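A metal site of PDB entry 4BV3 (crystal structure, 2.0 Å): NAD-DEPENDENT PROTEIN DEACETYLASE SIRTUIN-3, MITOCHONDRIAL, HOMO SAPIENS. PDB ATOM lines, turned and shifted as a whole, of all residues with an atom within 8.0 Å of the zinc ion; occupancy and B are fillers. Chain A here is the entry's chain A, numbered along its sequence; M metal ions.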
ATOM      1  N   THR A 140     -22.936 -23.948 -21.944  1.00  0.00           N
ATOM      2  CA  THR A 140     -24.366 -23.976 -21.741  1.00  0.00           C
ATOM      3  C   THR A 140     -25.120 -24.183 -23.042  1.00  0.00           C
ATOM      4  O   THR A 140     -24.810 -23.542 -24.045  1.00  0.00           O
ATOM      5  CB  THR A 140     -24.823 -22.668 -21.104  1.00  0.00           C
ATOM      6  OG1 THR A 140     -24.176 -22.455 -19.847  1.00  0.00           O
ATOM      7  CG2 THR A 140     -26.346 -22.682 -20.861  1.00  0.00           C
ATOM      8  N   CYS A 141     -26.106 -25.103 -23.046  1.00  0.00           N
ATOM      9  CA  CYS A 141     -26.960 -25.277 -24.183  1.00  0.00           C
ATOM     10  C   CYS A 141     -27.764 -23.996 -24.374  1.00  0.00           C
ATOM     11  O   CYS A 141     -28.442 -23.543 -23.460  1.00  0.00           O
ATOM     12  CB  CYS A 141     -27.931 -26.453 -23.992  1.00  0.00           C
ATOM     13  SG  CYS A 141     -29.009 -26.492 -25.421  1.00  0.00           S
ATOM     14  N   THR A 142     -27.667 -23.413 -25.567  1.00  0.00           N
ATOM     15  CA  THR A 142     -28.323 -22.159 -25.885  1.00  0.00           C
ATOM     16  C   THR A 142     -29.840 -22.280 -26.010  1.00  0.00           C
ATOM     17  O   THR A 142     -30.552 -21.264 -26.036  1.00  0.00           O
ATOM     18  CB  THR A 142     -27.818 -21.557 -27.245  1.00  0.00           C
ATOM     19  OG1 THR A 142     -28.051 -22.496 -28.297  1.00  0.00           O
ATOM     20  CG2 THR A 142     -26.353 -21.167 -27.198  1.00  0.00           C
ATOM     21  N   VAL A 143     -30.344 -23.504 -26.094  1.00  0.00           N
ATOM     22  CA  VAL A 143     -31.790 -23.756 -26.114  1.00  0.00           C
ATOM     23  C   VAL A 143     -32.342 -24.071 -24.727  1.00  0.00           C
ATOM     24  O   VAL A 143     -33.071 -23.244 -24.169  1.00  0.00           O
ATOM     25  CB  VAL A 143     -32.103 -24.897 -27.088  1.00  0.00           C
ATOM     26  CG1 VAL A 143     -33.507 -25.454 -26.855  1.00  0.00           C
ATOM     27  CG2 VAL A 143     -31.908 -24.425 -28.526  1.00  0.00           C
ATOM     28  N   CYS A 144     -32.005 -25.240 -24.175  1.00  0.00           N
ATOM     29  CA  CYS A 144     -32.551 -25.754 -22.883  1.00  0.00           C
ATOM     30  C   CYS A 144     -31.798 -25.313 -21.589  1.00  0.00           C
ATOM     31  O   CYS A 144     -32.173 -25.703 -20.501  1.00  0.00           O
ATOM     32  CB  CYS A 144     -32.572 -27.277 -22.899  1.00  0.00           C
ATOM     33  SG  CYS A 144     -30.981 -28.128 -22.645  1.00  0.00           S
ATOM     34  N   GLN A 145     -30.715 -24.557 -21.751  1.00  0.00           N
ATOM     35  CA  GLN A 145     -29.998 -23.967 -20.661  1.00  0.00           C
ATOM     36  C   GLN A 145     -29.324 -25.001 -19.796  1.00  0.00           C
ATOM     37  O   GLN A 145     -28.798 -24.661 -18.749  1.00  0.00           O
ATOM     38  CB  GLN A 145     -30.882 -23.063 -19.809  1.00  0.00           C
ATOM     39  CG  GLN A 145     -31.673 -22.010 -20.575  1.00  0.00           C
ATOM     40  CD  GLN A 145     -30.804 -21.141 -21.468  1.00  0.00           C
ATOM     41  OE1 GLN A 145     -29.716 -20.697 -21.077  1.00  0.00           O
ATOM     42  NE2 GLN A 145     -31.273 -20.892 -22.672  1.00  0.00           N
ATOM     43  N   ARG A 146     -29.233 -26.237 -20.251  1.00  0.00           N
ATOM     44  CA  ARG A 146     -28.437 -27.202 -19.533  1.00  0.00           C
ATOM     45  C   ARG A 146     -26.914 -26.877 -19.533  1.00  0.00           C
ATOM     46  O   ARG A 146     -26.290 -26.704 -20.593  1.00  0.00           O
ATOM     47  CB  ARG A 146     -28.716 -28.596 -20.026  1.00  0.00           C
ATOM     48  CG  ARG A 146     -27.981 -29.658 -19.247  1.00  0.00           C
ATOM     49  CD  ARG A 146     -28.538 -31.052 -19.570  1.00  0.00           C
ATOM     50  NE  ARG A 146     -27.909 -32.098 -18.733  1.00  0.00           N
ATOM     51  CZ  ARG A 146     -28.299 -32.447 -17.507  1.00  0.00           C
ATOM     52  NH1 ARG A 146     -29.316 -31.869 -16.910  1.00  0.00           N
ATOM     53  NH2 ARG A 146     -27.626 -33.394 -16.869  1.00  0.00           N
ATOM     54  N   PRO A 147     -26.315 -26.790 -18.321  1.00  0.00           N
ATOM     55  CA  PRO A 147     -24.874 -26.512 -18.200  1.00  0.00           C
ATOM     56  C   PRO A 147     -23.993 -27.760 -18.404  1.00  0.00           C
ATOM     57  O   PRO A 147     -24.437 -28.882 -18.110  1.00  0.00           O
ATOM     58  CB  PRO A 147     -24.713 -25.958 -16.767  1.00  0.00           C
ATOM     59  CG  PRO A 147     -26.007 -26.131 -16.079  1.00  0.00           C
ATOM     60  CD  PRO A 147     -26.978 -26.859 -16.993  1.00  0.00           C
ATOM     61  N   PHE A 148     -22.785 -27.567 -18.917  1.00  0.00           N
ATOM     62  CA  PHE A 148     -21.808 -28.640 -19.088  1.00  0.00           C
ATOM     63  C   PHE A 148     -20.466 -28.152 -18.662  1.00  0.00           C
ATOM     64  O   PHE A 148     -20.179 -26.976 -18.822  1.00  0.00           O
ATOM     65  CB  PHE A 148     -21.751 -29.116 -20.551  1.00  0.00           C
ATOM     66  CG  PHE A 148     -23.081 -29.553 -21.096  1.00  0.00           C
ATOM     67  CD1 PHE A 148     -23.554 -30.844 -20.891  1.00  0.00           C
ATOM     68  CD2 PHE A 148     -23.873 -28.661 -21.822  1.00  0.00           C
ATOM     69  CE1 PHE A 148     -24.788 -31.249 -21.415  1.00  0.00           C
ATOM     70  CE2 PHE A 148     -25.087 -29.040 -22.349  1.00  0.00           C
ATOM     71  CZ  PHE A 148     -25.568 -30.334 -22.155  1.00  0.00           C
ATOM     72  N   ARG A 164     -23.120 -29.893 -29.978  1.00  0.00           N
ATOM     73  CA  ARG A 164     -24.537 -29.972 -29.762  1.00  0.00           C
ATOM     74  C   ARG A 164     -24.969 -30.621 -28.455  1.00  0.00           C
ATOM     75  O   ARG A 164     -24.283 -31.448 -27.896  1.00  0.00           O
ATOM     76  CB  ARG A 164     -25.219 -30.644 -30.949  1.00  0.00           C
ATOM     77  CG  ARG A 164     -25.296 -29.637 -32.087  1.00  0.00           C
ATOM     78  CD  ARG A 164     -26.194 -30.100 -33.197  1.00  0.00           C
ATOM     79  NE  ARG A 164     -26.126 -29.077 -34.218  1.00  0.00           N
ATOM     80  CZ  ARG A 164     -26.922 -28.021 -34.313  1.00  0.00           C
ATOM     81  NH1 ARG A 164     -27.919 -27.787 -33.453  1.00  0.00           N
ATOM     82  NH2 ARG A 164     -26.707 -27.187 -35.290  1.00  0.00           N
ATOM     83  N   CYS A 165     -26.143 -30.201 -27.969  1.00  0.00           N
ATOM     84  CA  CYS A 165     -26.632 -30.668 -26.669  1.00  0.00           C
ATOM     85  C   CYS A 165     -27.171 -32.081 -26.840  1.00  0.00           C
ATOM     86  O   CYS A 165     -27.921 -32.338 -27.760  1.00  0.00           O
ATOM     87  CB  CYS A 165     -27.749 -29.740 -26.158  1.00  0.00           C
ATOM     88  SG  CYS A 165     -28.630 -30.256 -24.666  1.00  0.00           S
ATOM     89  N   PRO A 166     -26.794 -32.995 -25.959  1.00  0.00           N
ATOM     90  CA  PRO A 166     -27.266 -34.369 -26.081  1.00  0.00           C
ATOM     91  C   PRO A 166     -28.669 -34.608 -25.564  1.00  0.00           C
ATOM     92  O   PRO A 166     -29.139 -35.725 -25.658  1.00  0.00           O
ATOM     93  CB  PRO A 166     -26.298 -35.113 -25.184  1.00  0.00           C
ATOM     94  CG  PRO A 166     -26.070 -34.132 -24.105  1.00  0.00           C
ATOM     95  CD  PRO A 166     -25.848 -32.867 -24.844  1.00  0.00           C
ATOM     96  N   VAL A 167     -29.292 -33.589 -24.966  1.00  0.00           N
ATOM     97  CA  VAL A 167     -30.651 -33.663 -24.501  1.00  0.00           C
ATOM     98  C   VAL A 167     -31.572 -33.142 -25.594  1.00  0.00           C
ATOM     99  O   VAL A 167     -32.617 -33.733 -25.856  1.00  0.00           O
ATOM    100  CB  VAL A 167     -30.896 -32.782 -23.231  1.00  0.00           C
ATOM    101  CG1 VAL A 167     -32.342 -32.884 -22.752  1.00  0.00           C
ATOM    102  CG2 VAL A 167     -29.960 -33.161 -22.120  1.00  0.00           C
ATOM    103  N   CYS A 168     -31.197 -32.037 -26.213  1.00  0.00           N
ATOM    104  CA  CYS A 168     -32.129 -31.258 -27.005  1.00  0.00           C
ATOM    105  C   CYS A 168     -31.624 -30.880 -28.387  1.00  0.00           C
ATOM    106  O   CYS A 168     -32.388 -30.276 -29.171  1.00  0.00           O
ATOM    107  CB  CYS A 168     -32.536 -30.006 -26.200  1.00  0.00           C
ATOM    108  SG  CYS A 168     -31.643 -28.466 -26.489  1.00  0.00           S
ATOM    109  N   THR A 169     -30.353 -31.214 -28.675  1.00  0.00           N
ATOM    110  CA  THR A 169     -29.662 -30.964 -29.943  1.00  0.00           C
ATOM    111  C   THR A 169     -29.354 -29.492 -30.239  1.00  0.00           C
ATOM    112  O   THR A 169     -28.745 -29.176 -31.269  1.00  0.00           O
ATOM    113  CB  THR A 169     -30.430 -31.571 -31.135  1.00  0.00           C
ATOM    114  OG1 THR A 169     -31.530 -30.726 -31.455  1.00  0.00           O
ATOM    115  CG2 THR A 169     -30.944 -32.984 -30.770  1.00  0.00           C
ATOM    116  N   GLY A 170     -29.743 -28.591 -29.343  1.00  0.00           N
ATOM    117  CA  GLY A 170     -29.403 -27.185 -29.518  1.00  0.00           C
ATOM    118  C   GLY A 170     -27.892 -26.971 -29.530  1.00  0.00           C
ATOM    119  O   GLY A 170     -27.113 -27.774 -29.014  1.00  0.00           O
ATOM    120  N   VAL A 171     -27.466 -25.883 -30.154  1.00  0.00           N
ATOM    121  CA  VAL A 171     -26.027 -25.515 -30.074  1.00  0.00           C
ATOM    122  C   VAL A 171     -25.564 -25.208 -28.650  1.00  0.00           C
ATOM    123  O   VAL A 171     -26.162 -24.357 -27.941  1.00  0.00           O
ATOM    124  CB  VAL A 171     -25.702 -24.353 -31.054  1.00  0.00           C
ATOM    125  CG1 VAL A 171     -24.261 -23.864 -30.880  1.00  0.00           C
ATOM    126  CG2 VAL A 171     -25.951 -24.862 -32.502  1.00  0.00           C
ATOM    127  N   VAL A 172     -24.492 -25.887 -28.211  1.00  0.00           N
ATOM    128  CA  VAL A 172     -23.864 -25.599 -26.928  1.00  0.00           C
ATOM    129  C   VAL A 172     -22.723 -24.603 -27.042  1.00  0.00           C
ATOM    130  O   VAL A 172     -21.802 -24.796 -27.827  1.00  0.00           O
ATOM    131  CB  VAL A 172     -23.355 -26.882 -26.212  1.00  0.00           C
ATOM    132  CG1 VAL A 172     -22.723 -26.536 -24.897  1.00  0.00           C
ATOM    133  CG2 VAL A 172     -24.508 -27.842 -25.952  1.00  0.00           C
HETATM  134 ZN    ZN M   1     -30.128 -28.527 -24.799  1.00  0.00          ZN
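The side-chain sulfur of Cys 168 lies close to the backbone NH of Gly 170 (3.4 Å).
The backbone NH (N) of Cys 165 sits at hydrogen-bond distance from the backbone carbonyl oxygen (O) of Gly 170 (2.8 Å).
N of Val 167 lies close to SG of Cys 165 (3.4 Å).
The side-chain sulfur (SG) of Cys 144 lies close to the backbone NH (N) of Arg 146.
SG of Cys 141 lies close to N of Val 143.
N of Cys 141 sits at hydrogen-bond distance from O of Arg 146.
SG of Cys 168 is bound to the zinc ion, 2.3 Å away.
SG of Cys 165 is bound to the zinc ion (2.3 Å).
The zinc ion is bound by SG of Cys 144 (2.4 Å).
The zinc ion is bound by SG of Cys 141, at 2.4 Å.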
